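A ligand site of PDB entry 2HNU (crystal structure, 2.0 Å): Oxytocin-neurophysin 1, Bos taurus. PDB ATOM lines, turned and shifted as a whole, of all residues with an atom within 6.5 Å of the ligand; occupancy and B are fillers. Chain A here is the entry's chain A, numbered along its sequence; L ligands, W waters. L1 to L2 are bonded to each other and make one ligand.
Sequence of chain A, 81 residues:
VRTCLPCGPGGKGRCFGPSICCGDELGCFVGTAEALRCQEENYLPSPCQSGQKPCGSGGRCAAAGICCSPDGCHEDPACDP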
ATOM      1  N   ARG A   2     -10.716  30.411 -11.741  1.00  0.00           N
ATOM      2  CA  ARG A   2      -9.907  30.458 -10.538  1.00  0.00           C
ATOM      3  C   ARG A   2      -8.595  29.708 -10.682  1.00  0.00           C
ATOM      4  O   ARG A   2      -8.466  28.808 -11.511  1.00  0.00           O
ATOM      5  CB  ARG A   2     -10.678  29.910  -9.320  1.00  0.00           C
ATOM      6  CG  ARG A   2     -10.935  28.414  -9.345  1.00  0.00           C
ATOM      7  CD  ARG A   2     -11.717  27.931  -8.098  1.00  0.00           C
ATOM      8  NE  ARG A   2     -12.170  26.549  -8.303  1.00  0.00           N
ATOM      9  CZ  ARG A   2     -11.426  25.476  -8.106  1.00  0.00           C
ATOM     10  NH1 ARG A   2     -10.175  25.584  -7.669  1.00  0.00           N
ATOM     11  NH2 ARG A   2     -11.897  24.273  -8.422  1.00  0.00           N
ATOM     12  N   CYS A   4      -5.878  27.112  -9.382  1.00  0.00           N
ATOM     13  CA  CYS A   4      -6.128  25.846  -8.693  1.00  0.00           C
ATOM     14  C   CYS A   4      -5.691  25.916  -7.224  1.00  0.00           C
ATOM     15  O   CYS A   4      -5.073  26.889  -6.807  1.00  0.00           O
ATOM     16  CB  CYS A   4      -5.406  24.709  -9.435  1.00  0.00           C
ATOM     17  SG  CYS A   4      -5.887  24.576 -11.201  1.00  0.00           S
ATOM     18  N   LEU A   5      -6.021  24.891  -6.459  1.00  0.00           N
ATOM     19  CA  LEU A   5      -5.681  24.841  -5.044  1.00  0.00           C
ATOM     20  C   LEU A   5      -4.216  25.096  -4.727  1.00  0.00           C
ATOM     21  O   LEU A   5      -3.329  24.693  -5.486  1.00  0.00           O
ATOM     22  CB  LEU A   5      -6.077  23.475  -4.462  1.00  0.00           C
ATOM     23  CG  LEU A   5      -7.567  23.138  -4.390  1.00  0.00           C
ATOM     24  CD1 LEU A   5      -7.755  21.686  -3.943  1.00  0.00           C
ATOM     25  CD2 LEU A   5      -8.252  24.091  -3.435  1.00  0.00           C
ATOM     26  N   CYS A  15      -1.426  24.038  -7.684  1.00  0.00           N
ATOM     27  CA  CYS A  15      -1.564  22.792  -8.429  1.00  0.00           C
ATOM     28  C   CYS A  15      -1.721  23.042  -9.927  1.00  0.00           C
ATOM     29  O   CYS A  15      -2.457  23.930 -10.337  1.00  0.00           O
ATOM     30  CB  CYS A  15      -2.765  22.026  -7.909  1.00  0.00           C
ATOM     31  SG  CYS A  15      -2.631  21.547  -6.161  1.00  0.00           S
ATOM     32  N   PHE A  16      -1.029  22.236 -10.731  1.00  0.00           N
ATOM     33  CA  PHE A  16      -1.103  22.345 -12.184  1.00  0.00           C
ATOM     34  C   PHE A  16      -1.699  21.074 -12.755  1.00  0.00           C
ATOM     35  O   PHE A  16      -1.946  20.969 -13.958  1.00  0.00           O
ATOM     36  CB  PHE A  16       0.279  22.576 -12.774  1.00  0.00           C
ATOM     37  CG  PHE A  16       0.733  24.003 -12.695  1.00  0.00           C
ATOM     38  CD1 PHE A  16       1.037  24.572 -11.467  1.00  0.00           C
ATOM     39  CD2 PHE A  16       0.806  24.790 -13.844  1.00  0.00           C
ATOM     40  CE1 PHE A  16       1.400  25.918 -11.370  1.00  0.00           C
ATOM     41  CE2 PHE A  16       1.162  26.135 -13.759  1.00  0.00           C
ATOM     42  CZ  PHE A  16       1.466  26.699 -12.523  1.00  0.00           C
ATOM     43  N   GLY A  17      -1.918  20.103 -11.873  1.00  0.00           N
ATOM     44  CA  GLY A  17      -2.488  18.820 -12.253  1.00  0.00           C
ATOM     45  C   GLY A  17      -2.713  17.997 -10.992  1.00  0.00           C
ATOM     46  O   GLY A  17      -2.238  18.364  -9.909  1.00  0.00           O
ATOM     47  N   PRO A  18      -3.420  16.861 -11.100  1.00  0.00           N
ATOM     48  CA  PRO A  18      -3.706  15.973  -9.956  1.00  0.00           C
ATOM     49  C   PRO A  18      -2.494  15.672  -9.073  1.00  0.00           C
ATOM     50  O   PRO A  18      -2.628  15.571  -7.854  1.00  0.00           O
ATOM     51  CB  PRO A  18      -4.269  14.727 -10.623  1.00  0.00           C
ATOM     52  CG  PRO A  18      -4.954  15.276 -11.831  1.00  0.00           C
ATOM     53  CD  PRO A  18      -3.953  16.282 -12.345  1.00  0.00           C
ATOM     54  N   SER A  19      -1.316  15.531  -9.675  1.00  0.00           N
ATOM     55  CA  SER A  19      -0.133  15.255  -8.868  1.00  0.00           C
ATOM     56  C   SER A  19       1.036  16.169  -9.209  1.00  0.00           C
ATOM     57  O   SER A  19       2.199  15.750  -9.189  1.00  0.00           O
ATOM     58  CB  SER A  19       0.265  13.775  -9.033  1.00  0.00           C
ATOM     59  OG  SER A  19       0.545  13.466 -10.383  1.00  0.00           O
ATOM     60  N   ILE A  20       0.722  17.427  -9.500  1.00  0.00           N
ATOM     61  CA  ILE A  20       1.762  18.385  -9.847  1.00  0.00           C
ATOM     62  C   ILE A  20       1.579  19.691  -9.102  1.00  0.00           C
ATOM     63  O   ILE A  20       0.569  20.386  -9.284  1.00  0.00           O
ATOM     64  CB  ILE A  20       1.781  18.689 -11.353  1.00  0.00           C
ATOM     65  CG1 ILE A  20       2.001  17.393 -12.144  1.00  0.00           C
ATOM     66  CG2 ILE A  20       2.887  19.714 -11.665  1.00  0.00           C
ATOM     67  CD1 ILE A  20       1.887  17.574 -13.643  1.00  0.00           C
ATOM     68  N   ALA A  35       2.417  17.363  -3.538  1.00  0.00           N
ATOM     69  CA  ALA A  35       1.351  17.475  -4.531  1.00  0.00           C
ATOM     70  C   ALA A  35       0.103  16.630  -4.269  1.00  0.00           C
ATOM     71  O   ALA A  35      -0.805  16.590  -5.114  1.00  0.00           O
ATOM     72  CB  ALA A  35       1.898  17.150  -5.907  1.00  0.00           C
ATOM     73  N   ARG A  37      -2.403  17.144  -2.205  1.00  0.00           N
ATOM     74  CA  ARG A  37      -3.643  17.921  -2.123  1.00  0.00           C
ATOM     75  C   ARG A  37      -4.194  18.260  -3.501  1.00  0.00           C
ATOM     76  O   ARG A  37      -5.376  18.550  -3.647  1.00  0.00           O
ATOM     77  CB  ARG A  37      -3.437  19.211  -1.333  1.00  0.00           C
ATOM     78  CG  ARG A  37      -4.735  20.025  -1.185  1.00  0.00           C
ATOM     79  CD  ARG A  37      -4.714  20.871   0.079  1.00  0.00           C
ATOM     80  NE  ARG A  37      -3.696  21.909   0.022  1.00  0.00           N
ATOM     81  CZ  ARG A  37      -3.039  22.363   1.082  1.00  0.00           C
ATOM     82  NH1 ARG A  37      -3.278  21.867   2.288  1.00  0.00           N
ATOM     83  NH2 ARG A  37      -2.135  23.320   0.938  1.00  0.00           N
ATOM     84  N   CYS A  38      -3.320  18.208  -4.501  1.00  0.00           N
ATOM     85  CA  CYS A  38      -3.706  18.521  -5.865  1.00  0.00           C
ATOM     86  C   CYS A  38      -4.717  17.533  -6.453  1.00  0.00           C
ATOM     87  O   CYS A  38      -5.393  17.841  -7.435  1.00  0.00           O
ATOM     88  CB  CYS A  38      -2.465  18.607  -6.745  1.00  0.00           C
ATOM     89  SG  CYS A  38      -1.347  19.976  -6.285  1.00  0.00           S
ATOM     90  N   GLN A  39      -4.821  16.351  -5.857  1.00  0.00           N
ATOM     91  CA  GLN A  39      -5.780  15.364  -6.343  1.00  0.00           C
ATOM     92  C   GLN A  39      -7.191  15.765  -5.922  1.00  0.00           C
ATOM     93  O   GLN A  39      -8.173  15.349  -6.532  1.00  0.00           O
ATOM     94  CB  GLN A  39      -5.508  13.960  -5.760  1.00  0.00           C
ATOM     95  CG  GLN A  39      -4.089  13.439  -5.961  1.00  0.00           C
ATOM     96  CD  GLN A  39      -3.966  11.951  -5.605  1.00  0.00           C
ATOM     97  OE1 GLN A  39      -4.303  11.076  -6.405  1.00  0.00           O
ATOM     98  NE2 GLN A  39      -3.503  11.672  -4.394  1.00  0.00           N
ATOM     99  N   GLU A  40      -7.283  16.574  -4.870  1.00  0.00           N
ATOM    100  CA  GLU A  40      -8.570  17.004  -4.348  1.00  0.00           C
ATOM    101  C   GLU A  40      -9.348  17.871  -5.335  1.00  0.00           C
ATOM    102  O   GLU A  40     -10.580  17.941  -5.283  1.00  0.00           O
ATOM    103  CB  GLU A  40      -8.377  17.735  -3.007  1.00  0.00           C
ATOM    104  CG  GLU A  40      -7.657  16.882  -1.970  1.00  0.00           C
ATOM    105  CD  GLU A  40      -8.325  15.526  -1.769  1.00  0.00           C
ATOM    106  OE1 GLU A  40      -9.458  15.479  -1.231  1.00  0.00           O
ATOM    107  OE2 GLU A  40      -7.717  14.506  -2.141  1.00  0.00           O
ATOM    108  N   GLU A  41      -8.616  18.518  -6.225  1.00  0.00           N
ATOM    109  CA  GLU A  41      -9.213  19.379  -7.246  1.00  0.00           C
ATOM    110  C   GLU A  41     -10.182  18.557  -8.102  1.00  0.00           C
ATOM    111  O   GLU A  41     -11.155  19.088  -8.640  1.00  0.00           O
ATOM    112  CB  GLU A  41      -8.087  19.975  -8.103  1.00  0.00           C
ATOM    113  CG  GLU A  41      -8.531  20.976  -9.147  1.00  0.00           C
ATOM    114  CD  GLU A  41      -9.204  22.192  -8.550  1.00  0.00           C
ATOM    115  OE1 GLU A  41     -10.381  22.398  -8.868  1.00  0.00           O
ATOM    116  OE2 GLU A  41      -8.570  22.949  -7.772  1.00  0.00           O
ATOM    117  N   ASN A  42      -9.915  17.259  -8.211  1.00  0.00           N
ATOM    118  CA  ASN A  42     -10.775  16.367  -8.991  1.00  0.00           C
ATOM    119  C   ASN A  42     -12.192  16.334  -8.450  1.00  0.00           C
ATOM    120  O   ASN A  42     -13.133  16.055  -9.204  1.00  0.00           O
ATOM    121  CB  ASN A  42     -10.192  14.945  -8.996  1.00  0.00           C
ATOM    122  CG  ASN A  42      -8.923  14.838  -9.823  1.00  0.00           C
ATOM    123  OD1 ASN A  42      -8.230  13.820  -9.776  1.00  0.00           O
ATOM    124  ND2 ASN A  42      -8.622  15.869 -10.593  1.00  0.00           N
ATOM    125  N   TYR A  43     -12.357  16.630  -7.156  1.00  0.00           N
ATOM    126  CA  TYR A  43     -13.665  16.645  -6.514  1.00  0.00           C
ATOM    127  C   TYR A  43     -14.405  17.987  -6.661  1.00  0.00           C
ATOM    128  O   TYR A  43     -15.612  18.067  -6.427  1.00  0.00           O
ATOM    129  CB  TYR A  43     -13.550  16.336  -5.024  1.00  0.00           C
ATOM    130  CG  TYR A  43     -12.947  14.985  -4.691  1.00  0.00           C
ATOM    131  CD1 TYR A  43     -11.635  14.888  -4.223  1.00  0.00           C
ATOM    132  CD2 TYR A  43     -13.698  13.825  -4.809  1.00  0.00           C
ATOM    133  CE1 TYR A  43     -11.089  13.653  -3.882  1.00  0.00           C
ATOM    134  CE2 TYR A  43     -13.167  12.577  -4.474  1.00  0.00           C
ATOM    135  CZ  TYR A  43     -11.855  12.497  -4.008  1.00  0.00           C
ATOM    136  OH  TYR A  43     -11.331  11.279  -3.678  1.00  0.00           O
ATOM    137  N   LEU A  44     -13.682  19.032  -7.039  1.00  0.00           N
ATOM    138  CA  LEU A  44     -14.295  20.353  -7.189  1.00  0.00           C
ATOM    139  C   LEU A  44     -14.909  20.476  -8.577  1.00  0.00           C
ATOM    140  O   LEU A  44     -14.214  20.370  -9.593  1.00  0.00           O
ATOM    141  CB  LEU A  44     -13.239  21.425  -6.944  1.00  0.00           C
ATOM    142  CG  LEU A  44     -12.440  21.282  -5.634  1.00  0.00           C
ATOM    143  CD1 LEU A  44     -11.590  22.529  -5.436  1.00  0.00           C
ATOM    144  CD2 LEU A  44     -13.388  21.100  -4.453  1.00  0.00           C
ATOM    145  N   PRO A  45     -16.225  20.740  -8.643  1.00  0.00           N
ATOM    146  CA  PRO A  45     -16.976  20.881  -9.899  1.00  0.00           C
ATOM    147  C   PRO A  45     -16.699  22.127 -10.746  1.00  0.00           C
ATOM    148  O   PRO A  45     -17.221  22.244 -11.851  1.00  0.00           O
ATOM    149  CB  PRO A  45     -18.429  20.798  -9.434  1.00  0.00           C
ATOM    150  CG  PRO A  45     -18.381  21.536  -8.121  1.00  0.00           C
ATOM    151  CD  PRO A  45     -17.099  21.021  -7.475  1.00  0.00           C
ATOM    152  N   SER A  46     -15.893  23.055 -10.233  1.00  0.00           N
ATOM    153  CA  SER A  46     -15.571  24.254 -10.995  1.00  0.00           C
ATOM    154  C   SER A  46     -14.192  24.119 -11.638  1.00  0.00           C
ATOM    155  O   SER A  46     -13.278  23.525 -11.062  1.00  0.00           O
ATOM    156  CB  SER A  46     -15.617  25.495 -10.092  1.00  0.00           C
ATOM    157  OG  SER A  46     -14.621  25.447  -9.086  1.00  0.00           O
ATOM    158  N   PRO A  47     -14.017  24.678 -12.846  1.00  0.00           N
ATOM    159  CA  PRO A  47     -12.718  24.586 -13.512  1.00  0.00           C
ATOM    160  C   PRO A  47     -11.676  25.475 -12.836  1.00  0.00           C
ATOM    161  O   PRO A  47     -12.012  26.488 -12.223  1.00  0.00           O
ATOM    162  CB  PRO A  47     -13.033  25.041 -14.936  1.00  0.00           C
ATOM    163  CG  PRO A  47     -14.089  26.094 -14.699  1.00  0.00           C
ATOM    164  CD  PRO A  47     -14.982  25.449 -13.649  1.00  0.00           C
ATOM    165  N   CYS A  48     -10.405  25.090 -12.948  1.00  0.00           N
ATOM    166  CA  CYS A  48      -9.317  25.880 -12.386  1.00  0.00           C
ATOM    167  C   CYS A  48      -8.170  25.851 -13.364  1.00  0.00           C
ATOM    168  O   CYS A  48      -8.102  24.976 -14.230  1.00  0.00           O
ATOM    169  CB  CYS A  48      -8.852  25.314 -11.035  1.00  0.00           C
ATOM    170  SG  CYS A  48      -7.787  23.829 -11.130  1.00  0.00           S
ATOM    171  N   GLN A  49      -7.269  26.811 -13.245  1.00  0.00           N
ATOM    172  CA  GLN A  49      -6.104  26.880 -14.105  1.00  0.00           C
ATOM    173  C   GLN A  49      -5.044  27.696 -13.393  1.00  0.00           C
ATOM    174  O   GLN A  49      -5.326  28.774 -12.876  1.00  0.00           O
ATOM    175  CB  GLN A  49      -6.441  27.506 -15.455  1.00  0.00           C
ATOM    176  CG  GLN A  49      -5.257  27.531 -16.403  1.00  0.00           C
ATOM    177  CD  GLN A  49      -5.627  27.963 -17.813  1.00  0.00           C
ATOM    178  OE1 GLN A  49      -6.054  29.096 -18.041  1.00  0.00           O
ATOM    179  NE2 GLN A  49      -5.453  27.055 -18.769  1.00  0.00           N
ATOM    180  N   SER A  50      -3.823  27.173 -13.373  1.00  0.00           N
ATOM    181  CA  SER A  50      -2.711  27.859 -12.725  1.00  0.00           C
ATOM    182  C   SER A  50      -1.724  28.373 -13.773  1.00  0.00           C
ATOM    183  O   SER A  50      -1.757  27.944 -14.916  1.00  0.00           O
ATOM    184  CB  SER A  50      -1.998  26.898 -11.755  1.00  0.00           C
ATOM    185  OG  SER A  50      -2.873  26.471 -10.724  1.00  0.00           O
ATOM    186  N   PRO A  70      -1.421  19.280 -17.077  1.00  0.00           N
ATOM    187  CA  PRO A  70      -1.933  18.445 -15.985  1.00  0.00           C
ATOM    188  C   PRO A  70      -1.273  17.081 -15.796  1.00  0.00           C
ATOM    189  O   PRO A  70      -1.428  16.461 -14.746  1.00  0.00           O
ATOM    190  CB  PRO A  70      -3.415  18.316 -16.315  1.00  0.00           C
ATOM    191  CG  PRO A  70      -3.714  19.619 -16.960  1.00  0.00           C
ATOM    192  CD  PRO A  70      -2.537  19.765 -17.903  1.00  0.00           C
HETATM  193  N1  LIG L   1     -11.836  21.106 -10.574  1.00  0.00           N
HETATM  194  C1  LIG L   1     -11.142  20.171 -11.518  1.00  0.00           C
HETATM  195  C2  LIG L   1     -10.247  20.961 -12.465  1.00  0.00           C
HETATM  196  O1  LIG L   1     -10.436  22.163 -12.650  1.00  0.00           O
HETATM  197  C3  LIG L   1     -12.184  19.362 -12.322  1.00  0.00           C
HETATM  198  C4  LIG L   1     -12.938  20.169 -13.349  1.00  0.00           C
HETATM  199  C5  LIG L   1     -12.434  20.317 -14.636  1.00  0.00           C
HETATM  200  C6  LIG L   1     -14.138  20.792 -13.023  1.00  0.00           C
HETATM  201  C7  LIG L   1     -13.124  21.077 -15.593  1.00  0.00           C
HETATM  202  C8  LIG L   1     -14.835  21.558 -13.976  1.00  0.00           C
HETATM  203  C9  LIG L   1     -14.330  21.700 -15.254  1.00  0.00           C
HETATM  204  N1  LG2 L   2      -9.264  20.292 -13.058  1.00  0.00           N
HETATM  205  C1  LG2 L   2      -8.335  20.969 -13.962  1.00  0.00           C
HETATM  206  C2  LG2 L   2      -8.937  21.179 -15.356  1.00  0.00           C
HETATM  207  O1  LG2 L   2      -9.002  22.357 -15.795  1.00  0.00           O
HETATM  208  C3  LG2 L   2      -7.026  20.169 -14.066  1.00  0.00           C
HETATM  209  C4  LG2 L   2      -6.331  20.026 -12.734  1.00  0.00           C
HETATM  210  C5  LG2 L   2      -6.483  18.870 -11.975  1.00  0.00           C
HETATM  211  C6  LG2 L   2      -5.615  21.095 -12.184  1.00  0.00           C
HETATM  212  C7  LG2 L   2      -5.956  18.786 -10.683  1.00  0.00           C
HETATM  213  C8  LG2 L   2      -5.090  21.022 -10.908  1.00  0.00           C
HETATM  214  C9  LG2 L   2      -5.264  19.864 -10.160  1.00  0.00           C
HETATM  215  O2  LG2 L   2      -4.774  19.815  -8.878  1.00  0.00           O
HETATM  216  O3  LG2 L   2      -9.326  20.180 -15.980  1.00  0.00           O
HETATM  217  O   HOH W   1      -9.580  17.468 -12.406  1.00  0.00           O
HETATM  218  O   HOH W   2      -5.880  23.276 -15.220  1.00  0.00           O
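The backbone carbonyl oxygen (O) of Cys 38 is in hydrogen-bond range of an oxygen (O2) of LG2 L2 (2.5 Å).
A nitrogen (N1) of LIG L1 sits at hydrogen-bond distance from the backbone carbonyl oxygen of Glu 41.
OE1 of Glu 41 lies within salt-bridge range of N1 of LIG L1 (2.6 Å).
O of Leu 44 lies within hydrogen-bond range of N1 of LIG L1 (2.7 Å).
O of Ser 46 sits at hydrogen-bond distance from N1 of LIG L1 (2.9 Å).
O1 of LIG L1 sits at hydrogen-bond distance from N of Cys 48 (2.9 Å).
O of Gly 17 lies within hydrogen-bond range of O2 of LG2 L2 (3.1 Å).
Merely in contact with the ligand: Arg 2 (3.8 Å), Cys 4 (3.6 Å), Cys 15 (3.1 Å), Phe 16 (3.9 Å), Pro 18 (3.2 Å), Asn 42 (3.9 Å), Pro 45 (3.3 Å) and Pro 47 (3.4 Å).
SG of Cys 38 is disulfide-bonded to SG of Cys 15 (2.0 Å).
NH2 of Arg 2 lies within salt-bridge range of OE1 of Glu 41 (2.5 Å).
The side-chain hydroxyl (OG) of Ser 46 is in hydrogen-bond range of the guanidinium group (NE) of Arg 2.
SG of Cys 48 is disulfide-bonded to SG of Cys 4 (2.0 Å).
N of Cys 15 sits at hydrogen-bond distance from O of Leu 5.
The backbone carbonyl oxygen (O) of Cys 15 sits at hydrogen-bond distance from the side-chain hydroxyl (OG) of Ser 50, at 2.6 Å.
N of Gln 39 is in hydrogen-bond range of O of Pro 18.
The backbone NH of Gln 49 lies within hydrogen-bond range of the backbone carbonyl oxygen of Arg 2, at 2.9 Å.
Water W1 bridges the side-chain amide nitrogen of Asn 42 and a nitrogen (N1) of LG2 L2.
Water W2 bridges O of Cys 48 and O1 of LG2 L2.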
